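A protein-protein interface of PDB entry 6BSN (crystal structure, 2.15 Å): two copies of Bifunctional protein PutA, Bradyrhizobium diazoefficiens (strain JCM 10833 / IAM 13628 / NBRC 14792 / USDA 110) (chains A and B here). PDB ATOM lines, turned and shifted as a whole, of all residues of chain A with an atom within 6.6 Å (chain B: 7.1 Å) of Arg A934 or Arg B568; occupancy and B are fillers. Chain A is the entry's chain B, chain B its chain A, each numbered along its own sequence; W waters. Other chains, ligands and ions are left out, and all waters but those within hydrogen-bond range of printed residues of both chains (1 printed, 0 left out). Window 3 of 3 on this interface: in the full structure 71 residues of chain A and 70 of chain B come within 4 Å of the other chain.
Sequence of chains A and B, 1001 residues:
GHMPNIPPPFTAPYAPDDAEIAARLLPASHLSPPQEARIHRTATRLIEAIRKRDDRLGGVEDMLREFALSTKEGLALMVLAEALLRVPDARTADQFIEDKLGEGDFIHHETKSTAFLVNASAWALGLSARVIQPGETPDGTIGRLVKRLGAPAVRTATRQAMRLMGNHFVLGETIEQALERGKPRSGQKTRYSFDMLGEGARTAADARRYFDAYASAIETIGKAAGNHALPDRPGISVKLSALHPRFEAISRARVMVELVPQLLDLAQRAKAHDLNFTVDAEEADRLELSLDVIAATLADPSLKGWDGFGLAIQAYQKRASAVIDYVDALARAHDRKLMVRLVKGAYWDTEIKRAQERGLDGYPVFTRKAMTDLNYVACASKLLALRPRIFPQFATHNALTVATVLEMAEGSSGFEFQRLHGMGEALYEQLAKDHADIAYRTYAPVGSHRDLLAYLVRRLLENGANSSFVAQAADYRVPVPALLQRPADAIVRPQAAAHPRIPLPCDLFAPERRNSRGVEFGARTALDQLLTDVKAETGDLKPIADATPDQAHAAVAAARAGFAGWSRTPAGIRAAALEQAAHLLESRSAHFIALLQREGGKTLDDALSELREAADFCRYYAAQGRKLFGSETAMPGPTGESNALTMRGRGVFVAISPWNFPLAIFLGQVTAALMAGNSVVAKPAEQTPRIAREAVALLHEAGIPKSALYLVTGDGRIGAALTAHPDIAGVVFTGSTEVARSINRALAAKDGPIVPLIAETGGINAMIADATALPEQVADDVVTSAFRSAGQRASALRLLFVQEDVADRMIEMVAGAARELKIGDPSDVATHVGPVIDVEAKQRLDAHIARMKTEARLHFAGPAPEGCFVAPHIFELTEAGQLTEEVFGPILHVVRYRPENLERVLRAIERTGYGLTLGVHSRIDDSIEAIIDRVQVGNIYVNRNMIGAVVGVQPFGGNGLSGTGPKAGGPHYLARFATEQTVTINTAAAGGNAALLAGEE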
ATOM      1  N   LEU A 902      12.491 -15.676  -9.304  1.00  0.00           N
ATOM      2  CA  LEU A 902      11.502 -14.691  -9.735  1.00  0.00           C
ATOM      3  C   LEU A 902      12.174 -13.436 -10.284  1.00  0.00           C
ATOM      4  O   LEU A 902      11.596 -12.736 -11.125  1.00  0.00           O
ATOM      5  CB  LEU A 902      10.557 -14.330  -8.591  1.00  0.00           C
ATOM      6  CG  LEU A 902       9.516 -13.235  -8.896  1.00  0.00           C
ATOM      7  CD1 LEU A 902       8.661 -13.584 -10.106  1.00  0.00           C
ATOM      8  CD2 LEU A 902       8.634 -12.999  -7.714  1.00  0.00           C
ATOM      9  N   GLU A 903      13.389 -13.139  -9.820  1.00  0.00           N
ATOM     10  CA  GLU A 903      14.130 -11.985 -10.321  1.00  0.00           C
ATOM     11  C   GLU A 903      14.470 -12.144 -11.797  1.00  0.00           C
ATOM     12  O   GLU A 903      14.395 -11.182 -12.573  1.00  0.00           O
ATOM     13  CB  GLU A 903      15.404 -11.798  -9.494  1.00  0.00           C
ATOM     14  CG  GLU A 903      16.381 -10.769 -10.045  1.00  0.00           C
ATOM     15  CD  GLU A 903      15.843  -9.362  -9.944  1.00  0.00           C
ATOM     16  OE1 GLU A 903      14.876  -9.154  -9.174  1.00  0.00           O
ATOM     17  OE2 GLU A 903      16.382  -8.471 -10.634  1.00  0.00           O
ATOM     18  N   LEU A 906      11.315 -11.370 -13.751  1.00  0.00           N
ATOM     19  CA  LEU A 906      11.025  -9.949 -13.842  1.00  0.00           C
ATOM     20  C   LEU A 906      11.990  -9.249 -14.795  1.00  0.00           C
ATOM     21  O   LEU A 906      11.578  -8.373 -15.556  1.00  0.00           O
ATOM     22  CB  LEU A 906      11.076  -9.337 -12.448  1.00  0.00           C
ATOM     23  CG  LEU A 906       9.995  -9.879 -11.509  1.00  0.00           C
ATOM     24  CD1 LEU A 906      10.236  -9.381 -10.104  1.00  0.00           C
ATOM     25  CD2 LEU A 906       8.617  -9.469 -12.000  1.00  0.00           C
ATOM     26  N   ARG A 907      13.262  -9.654 -14.797  1.00  0.00           N
ATOM     27  CA  ARG A 907      14.211  -9.117 -15.769  1.00  0.00           C
ATOM     28  C   ARG A 907      13.830  -9.498 -17.193  1.00  0.00           C
ATOM     29  O   ARG A 907      13.974  -8.690 -18.117  1.00  0.00           O
ATOM     30  CB  ARG A 907      15.620  -9.616 -15.453  1.00  0.00           C
ATOM     31  CG  ARG A 907      16.373  -8.718 -14.508  1.00  0.00           C
ATOM     32  CD  ARG A 907      17.827  -9.093 -14.487  1.00  0.00           C
ATOM     33  NE  ARG A 907      18.321  -9.228 -13.124  1.00  0.00           N
ATOM     34  CZ  ARG A 907      19.514  -9.721 -12.812  1.00  0.00           C
ATOM     35  NH1 ARG A 907      19.886  -9.808 -11.541  1.00  0.00           N
ATOM     36  NH2 ARG A 907      20.331 -10.130 -13.775  1.00  0.00           N
ATOM     37  N   GLU A 910      11.055  -7.145 -18.160  1.00  0.00           N
ATOM     38  CA  GLU A 910      11.595  -5.821 -18.461  1.00  0.00           C
ATOM     39  C   GLU A 910      12.324  -5.809 -19.802  1.00  0.00           C
ATOM     40  O   GLU A 910      12.268  -4.814 -20.536  1.00  0.00           O
ATOM     41  CB  GLU A 910      12.519  -5.366 -17.326  1.00  0.00           C
ATOM     42  CG  GLU A 910      11.767  -5.091 -15.998  1.00  0.00           C
ATOM     43  CD  GLU A 910      12.683  -4.705 -14.826  1.00  0.00           C
ATOM     44  OE1 GLU A 910      13.854  -5.154 -14.796  1.00  0.00           O
ATOM     45  OE2 GLU A 910      12.224  -3.955 -13.930  1.00  0.00           O
ATOM     46  N   GLU A 929       2.623  -7.824  -4.324  1.00  0.00           N
ATOM     47  CA  GLU A 929       3.089  -6.453  -4.139  1.00  0.00           C
ATOM     48  C   GLU A 929       4.523  -6.285  -4.625  1.00  0.00           C
ATOM     49  O   GLU A 929       4.859  -5.265  -5.244  1.00  0.00           O
ATOM     50  CB  GLU A 929       2.957  -6.048  -2.665  1.00  0.00           C
ATOM     51  CG  GLU A 929       1.524  -5.878  -2.224  1.00  0.00           C
ATOM     52  CD  GLU A 929       1.359  -5.928  -0.707  1.00  0.00           C
ATOM     53  OE1 GLU A 929       2.380  -5.752   0.001  1.00  0.00           O
ATOM     54  OE2 GLU A 929       0.214  -6.144  -0.233  1.00  0.00           O
ATOM     55  N   ALA A 930       5.385  -7.271  -4.354  1.00  0.00           N
ATOM     56  CA  ALA A 930       6.761  -7.211  -4.841  1.00  0.00           C
ATOM     57  C   ALA A 930       6.818  -7.122  -6.365  1.00  0.00           C
ATOM     58  O   ALA A 930       7.692  -6.444  -6.918  1.00  0.00           O
ATOM     59  CB  ALA A 930       7.538  -8.428  -4.358  1.00  0.00           C
ATOM     60  N   ILE A 931       5.910  -7.818  -7.059  1.00  0.00           N
ATOM     61  CA  ILE A 931       5.876  -7.758  -8.519  1.00  0.00           C
ATOM     62  C   ILE A 931       5.404  -6.385  -8.980  1.00  0.00           C
ATOM     63  O   ILE A 931       6.014  -5.765  -9.858  1.00  0.00           O
ATOM     64  CB  ILE A 931       4.998  -8.888  -9.089  1.00  0.00           C
ATOM     65  CG1 ILE A 931       5.690 -10.246  -8.887  1.00  0.00           C
ATOM     66  CG2 ILE A 931       4.731  -8.647 -10.566  1.00  0.00           C
ATOM     67  CD1 ILE A 931       4.837 -11.486  -9.233  1.00  0.00           C
ATOM     68  N   ILE A 932       4.329  -5.879  -8.369  1.00  0.00           N
ATOM     69  CA  ILE A 932       3.785  -4.576  -8.736  1.00  0.00           C
ATOM     70  C   ILE A 932       4.829  -3.488  -8.537  1.00  0.00           C
ATOM     71  O   ILE A 932       4.968  -2.581  -9.367  1.00  0.00           O
ATOM     72  CB  ILE A 932       2.513  -4.283  -7.916  1.00  0.00           C
ATOM     73  CG1 ILE A 932       1.354  -5.183  -8.354  1.00  0.00           C
ATOM     74  CG2 ILE A 932       2.129  -2.837  -8.027  1.00  0.00           C
ATOM     75  CD1 ILE A 932       0.202  -5.172  -7.381  1.00  0.00           C
ATOM     76  N   ASP A 933       5.571  -3.558  -7.430  1.00  0.00           N
ATOM     77  CA  ASP A 933       6.581  -2.548  -7.134  1.00  0.00           C
ATOM     78  C   ASP A 933       7.697  -2.559  -8.169  1.00  0.00           C
ATOM     79  O   ASP A 933       8.258  -1.506  -8.488  1.00  0.00           O
ATOM     80  CB  ASP A 933       7.126  -2.775  -5.715  1.00  0.00           C
ATOM     81  CG  ASP A 933       8.394  -1.967  -5.411  1.00  0.00           C
ATOM     82  OD1 ASP A 933       9.523  -2.487  -5.627  1.00  0.00           O
ATOM     83  OD2 ASP A 933       8.258  -0.815  -4.937  1.00  0.00           O
ATOM     84  N   ARG A 934       8.010  -3.730  -8.722  1.00  0.00           N
ATOM     85  CA  ARG A 934       9.171  -3.877  -9.591  1.00  0.00           C
ATOM     86  C   ARG A 934       8.883  -3.490 -11.046  1.00  0.00           C
ATOM     87  O   ARG A 934       9.721  -2.845 -11.685  1.00  0.00           O
ATOM     88  CB  ARG A 934       9.689  -5.310  -9.505  1.00  0.00           C
ATOM     89  CG  ARG A 934      10.663  -5.668 -10.605  1.00  0.00           C
ATOM     90  CD  ARG A 934      11.970  -4.916 -10.444  1.00  0.00           C
ATOM     91  NE  ARG A 934      12.960  -5.358 -11.418  1.00  0.00           N
ATOM     92  CZ  ARG A 934      13.884  -6.270 -11.155  1.00  0.00           C
ATOM     93  NH1 ARG A 934      14.748  -6.625 -12.092  1.00  0.00           N
ATOM     94  NH2 ARG A 934      13.942  -6.829  -9.949  1.00  0.00           N
ATOM     95  N   VAL A 935       7.726  -3.887 -11.596  1.00  0.00           N
ATOM     96  CA  VAL A 935       7.448  -3.705 -13.020  1.00  0.00           C
ATOM     97  C   VAL A 935       6.847  -2.323 -13.270  1.00  0.00           C
ATOM     98  O   VAL A 935       6.324  -1.660 -12.370  1.00  0.00           O
ATOM     99  CB  VAL A 935       6.513  -4.805 -13.555  1.00  0.00           C
ATOM    100  CG1 VAL A 935       6.992  -6.154 -13.128  1.00  0.00           C
ATOM    101  CG2 VAL A 935       5.090  -4.571 -13.086  1.00  0.00           C
ATOM    102  N   GLN A 936       6.907  -1.879 -14.522  1.00  0.00           N
ATOM    103  CA  GLN A 936       6.348  -0.588 -14.898  1.00  0.00           C
ATOM    104  C   GLN A 936       5.074  -0.712 -15.725  1.00  0.00           C
ATOM    105  O   GLN A 936       4.470   0.307 -16.087  1.00  0.00           O
ATOM    106  CB  GLN A 936       7.397   0.223 -15.656  1.00  0.00           C
ATOM    107  CG  GLN A 936       8.288   1.011 -14.741  1.00  0.00           C
ATOM    108  CD  GLN A 936       9.184   1.963 -15.490  1.00  0.00           C
ATOM    109  OE1 GLN A 936      10.041   1.549 -16.269  1.00  0.00           O
ATOM    110  NE2 GLN A 936       8.984   3.259 -15.261  1.00  0.00           N
ATOM    111  N   GLY B 562      20.277   5.094 -10.338  1.00  0.00           N
ATOM    112  CA  GLY B 562      19.603   5.674  -9.191  1.00  0.00           C
ATOM    113  C   GLY B 562      18.103   5.807  -9.338  1.00  0.00           C
ATOM    114  O   GLY B 562      17.422   6.126  -8.357  1.00  0.00           O
ATOM    115  N   PHE B 563      17.578   5.546 -10.538  1.00  0.00           N
ATOM    116  CA  PHE B 563      16.163   5.766 -10.810  1.00  0.00           C
ATOM    117  C   PHE B 563      15.274   4.899  -9.918  1.00  0.00           C
ATOM    118  O   PHE B 563      14.293   5.388  -9.340  1.00  0.00           O
ATOM    119  CB  PHE B 563      15.869   5.499 -12.288  1.00  0.00           C
ATOM    120  CG  PHE B 563      14.405   5.326 -12.584  1.00  0.00           C
ATOM    121  CD1 PHE B 563      13.509   6.359 -12.354  1.00  0.00           C
ATOM    122  CD2 PHE B 563      13.922   4.119 -13.058  1.00  0.00           C
ATOM    123  CE1 PHE B 563      12.155   6.194 -12.603  1.00  0.00           C
ATOM    124  CE2 PHE B 563      12.562   3.938 -13.315  1.00  0.00           C
ATOM    125  CZ  PHE B 563      11.679   4.981 -13.087  1.00  0.00           C
ATOM    126  N   ALA B 564      15.576   3.596  -9.840  1.00  0.00           N
ATOM    127  CA  ALA B 564      14.712   2.638  -9.144  1.00  0.00           C
ATOM    128  C   ALA B 564      14.441   3.052  -7.703  1.00  0.00           C
ATOM    129  O   ALA B 564      13.285   3.081  -7.262  1.00  0.00           O
ATOM    130  CB  ALA B 564      15.342   1.239  -9.184  1.00  0.00           C
ATOM    131  N   GLY B 565      15.498   3.373  -6.953  1.00  0.00           N
ATOM    132  CA  GLY B 565      15.314   3.765  -5.567  1.00  0.00           C
ATOM    133  C   GLY B 565      14.610   5.106  -5.401  1.00  0.00           C
ATOM    134  O   GLY B 565      13.764   5.265  -4.520  1.00  0.00           O
ATOM    135  N   TRP B 566      14.941   6.088  -6.233  1.00  0.00           N
ATOM    136  CA  TRP B 566      14.261   7.377  -6.106  1.00  0.00           C
ATOM    137  C   TRP B 566      12.796   7.243  -6.462  1.00  0.00           C
ATOM    138  O   TRP B 566      11.929   7.714  -5.721  1.00  0.00           O
ATOM    139  CB  TRP B 566      14.920   8.428  -6.992  1.00  0.00           C
ATOM    140  CG  TRP B 566      14.308   9.784  -6.857  1.00  0.00           C
ATOM    141  CD1 TRP B 566      13.688  10.513  -7.837  1.00  0.00           C
ATOM    142  CD2 TRP B 566      14.241  10.575  -5.671  1.00  0.00           C
ATOM    143  NE1 TRP B 566      13.261  11.712  -7.337  1.00  0.00           N
ATOM    144  CE2 TRP B 566      13.588  11.778  -6.010  1.00  0.00           C
ATOM    145  CE3 TRP B 566      14.689  10.394  -4.361  1.00  0.00           C
ATOM    146  CZ2 TRP B 566      13.365  12.790  -5.088  1.00  0.00           C
ATOM    147  CZ3 TRP B 566      14.451  11.390  -3.442  1.00  0.00           C
ATOM    148  CH2 TRP B 566      13.805  12.579  -3.812  1.00  0.00           C
ATOM    149  N   SER B 567      12.507   6.531  -7.555  1.00  0.00           N
ATOM    150  CA  SER B 567      11.130   6.267  -7.951  1.00  0.00           C
ATOM    151  C   SER B 567      10.319   5.647  -6.818  1.00  0.00           C
ATOM    152  O   SER B 567       9.130   5.954  -6.660  1.00  0.00           O
ATOM    153  CB  SER B 567      11.114   5.343  -9.162  1.00  0.00           C
ATOM    154  OG  SER B 567       9.785   5.120  -9.591  1.00  0.00           O
ATOM    155  N   ARG B 568      10.934   4.757  -6.032  1.00  0.00           N
ATOM    156  CA  ARG B 568      10.243   4.065  -4.949  1.00  0.00           C
ATOM    157  C   ARG B 568      10.305   4.809  -3.617  1.00  0.00           C
ATOM    158  O   ARG B 568       9.647   4.385  -2.656  1.00  0.00           O
ATOM    159  CB  ARG B 568      10.819   2.654  -4.799  1.00  0.00           C
ATOM    160  CG  ARG B 568      10.385   1.741  -5.932  1.00  0.00           C
ATOM    161  CD  ARG B 568      11.053   0.355  -5.868  1.00  0.00           C
ATOM    162  NE  ARG B 568      10.798  -0.447  -7.076  1.00  0.00           N
ATOM    163  CZ  ARG B 568      11.155  -0.105  -8.322  1.00  0.00           C
ATOM    164  NH1 ARG B 568      10.875  -0.913  -9.340  1.00  0.00           N
ATOM    165  NH2 ARG B 568      11.778   1.045  -8.568  1.00  0.00           N
ATOM    166  N   THR B 569      11.046   5.913  -3.540  1.00  0.00           N
ATOM    167  CA  THR B 569      11.006   6.753  -2.348  1.00  0.00           C
ATOM    168  C   THR B 569       9.624   7.385  -2.198  1.00  0.00           C
ATOM    169  O   THR B 569       9.085   7.918  -3.174  1.00  0.00           O
ATOM    170  CB  THR B 569      12.077   7.830  -2.440  1.00  0.00           C
ATOM    171  OG1 THR B 569      13.352   7.195  -2.533  1.00  0.00           O
ATOM    172  CG2 THR B 569      12.044   8.749  -1.216  1.00  0.00           C
ATOM    173  N   PRO B 570       9.022   7.342  -1.006  1.00  0.00           N
ATOM    174  CA  PRO B 570       7.663   7.888  -0.832  1.00  0.00           C
ATOM    175  C   PRO B 570       7.550   9.357  -1.233  1.00  0.00           C
ATOM    176  O   PRO B 570       8.466  10.154  -1.012  1.00  0.00           O
ATOM    177  CB  PRO B 570       7.391   7.692   0.665  1.00  0.00           C
ATOM    178  CG  PRO B 570       8.296   6.492   1.047  1.00  0.00           C
ATOM    179  CD  PRO B 570       9.512   6.621   0.189  1.00  0.00           C
ATOM    180  N   ALA B 571       6.400   9.700  -1.830  1.00  0.00           N
ATOM    181  CA  ALA B 571       6.163  11.050  -2.358  1.00  0.00           C
ATOM    182  C   ALA B 571       6.359  12.132  -1.299  1.00  0.00           C
ATOM    183  O   ALA B 571       6.870  13.221  -1.596  1.00  0.00           O
ATOM    184  CB  ALA B 571       4.753  11.145  -2.931  1.00  0.00           C
ATOM    185  N   ARG B 574      10.024  12.812  -1.075  1.00  0.00           N
ATOM    186  CA  ARG B 574      10.449  13.651  -2.191  1.00  0.00           C
ATOM    187  C   ARG B 574       9.982  15.084  -1.982  1.00  0.00           C
ATOM    188  O   ARG B 574      10.761  16.026  -2.164  1.00  0.00           O
ATOM    189  CB  ARG B 574       9.934  13.077  -3.523  1.00  0.00           C
ATOM    190  CG  ARG B 574      10.260  11.555  -3.668  1.00  0.00           C
ATOM    191  CD  ARG B 574      10.242  11.062  -5.109  1.00  0.00           C
ATOM    192  NE  ARG B 574       8.972  11.272  -5.799  1.00  0.00           N
ATOM    193  CZ  ARG B 574       8.036  10.336  -5.971  1.00  0.00           C
ATOM    194  NH1 ARG B 574       8.195   9.106  -5.486  1.00  0.00           N
ATOM    195  NH2 ARG B 574       6.932  10.631  -6.632  1.00  0.00           N
ATOM    196  N   ARG B 648       3.701   6.953 -11.641  1.00  0.00           N
ATOM    197  CA  ARG B 648       5.045   6.700 -11.149  1.00  0.00           C
ATOM    198  C   ARG B 648       6.059   7.306 -12.101  1.00  0.00           C
ATOM    199  O   ARG B 648       5.751   7.626 -13.253  1.00  0.00           O
ATOM    200  CB  ARG B 648       5.291   5.193 -10.938  1.00  0.00           C
ATOM    201  CG  ARG B 648       4.875   4.299 -12.087  1.00  0.00           C
ATOM    202  CD  ARG B 648       4.758   2.819 -11.629  1.00  0.00           C
ATOM    203  NE  ARG B 648       6.030   2.201 -11.246  1.00  0.00           N
ATOM    204  CZ  ARG B 648       6.150   1.048 -10.568  1.00  0.00           C
ATOM    205  NH1 ARG B 648       7.356   0.565 -10.279  1.00  0.00           N
ATOM    206  NH2 ARG B 648       5.076   0.380 -10.147  1.00  0.00           N
ATOM    207  N   GLY B 677       9.338  11.417  -9.473  1.00  0.00           N
ATOM    208  CA  GLY B 677       9.986  10.140  -9.261  1.00  0.00           C
ATOM    209  C   GLY B 677      11.036   9.766 -10.283  1.00  0.00           C
ATOM    210  O   GLY B 677      11.455   8.605 -10.319  1.00  0.00           O
ATOM    211  N   GLN B 981      -0.473   3.850 -13.863  1.00  0.00           N
ATOM    212  CA  GLN B 981      -0.543   2.414 -13.625  1.00  0.00           C
ATOM    213  C   GLN B 981      -1.893   2.065 -13.020  1.00  0.00           C
ATOM    214  O   GLN B 981      -2.313   2.660 -12.023  1.00  0.00           O
ATOM    215  CB  GLN B 981       0.592   1.948 -12.710  1.00  0.00           C
ATOM    216  CG  GLN B 981       0.570   0.480 -12.400  1.00  0.00           C
ATOM    217  CD  GLN B 981       1.916  -0.002 -11.936  1.00  0.00           C
ATOM    218  OE1 GLN B 981       2.273   0.171 -10.778  1.00  0.00           O
ATOM    219  NE2 GLN B 981       2.689  -0.597 -12.851  1.00  0.00           N
HETATM  220  O   HOH W   1       8.348   3.948 -12.133  1.00  0.00           O
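O of Asp A933 sits at hydrogen-bond distance from NH1 of Arg B648 (2.9 Å). NH1 of Arg B568 is in hydrogen-bond range of O of Arg A934 (3.3 Å). The guanidinium group of Arg B568 lies within salt-bridge range of the side-chain carboxylate of Asp A933. The guanidinium group of Arg B648 lies within hydrogen-bond range of the backbone carbonyl oxygen of Ile A932 (3.1 Å). NH1 of Arg B648 lies within hydrogen-bond range of O of Val A935, at 3.2 Å.
O of Ala B564 lies within hydrogen-bond range of NH2 of Arg B568 (2.8 Å). OE1 of Glu A903 lies within salt-bridge range of NH2 of Arg A934, 2.6 Å away. The side-chain carboxylate of Glu A910 lies within salt-bridge range of the guanidinium group of Arg A934, at 3.0 Å. NH2 of Arg B648 is in hydrogen-bond range of OE1 of Gln B981.
Val A935 touches Gln B981 (O to NE2, 3.8 Å). NE2 of Gln A936 touches CZ of Phe B563 (3.9 Å). Gln A936 touches Gln B981 (C to NE2, 3.7 Å).
Arg A934 touches just one residue of chain B: Arg B568 (3.3 Å). Arg B568 touches two residues of chain A. Printed residues of chain B within 4 Å of Gln A936: Phe B563 (3.9 Å) and Gln B981 (3.7 Å). Of the printed residues of chain A, Gln B981 touches Val A935 and Gln A936. Printed residues of chain B within 4 Å of Ile A932: Arg B648. Of the printed residues of chain A, Phe B563 touches Gln A936. Trp B566 touches none of the printed residues of chain A. The nearest residue of chain B that does not touch Arg A934 is Arg B648 (4.4 Å).
Printed residues of chain A that touch a printed residue of chain B: Ile A932, Asp A933, Arg A934, Val A935 and Gln A936. Of the 14 printed residues of chain B, 4 touch a printed residue of chain A. Hydrophobic or aromatic side chains of chain B within 4 Å of the printed part of chain A: Phe B563. Among the printed residues, Asp or Glu carboxylates within 4 Å of a Lys or Arg side-chain nitrogen of the other chain: Asp A933 with Arg B568.
No position is printed for both chains. Of the 8 pairs that touch across the chains among the printed residues, none has its exchanged pair printed and touching as well.
Water W1 lies within hydrogen-bond range of NE of Arg B648 (3.0 Å), OG of Ser B567 (3.1 Å) and NE2 of Gln A936 (3.3 Å).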
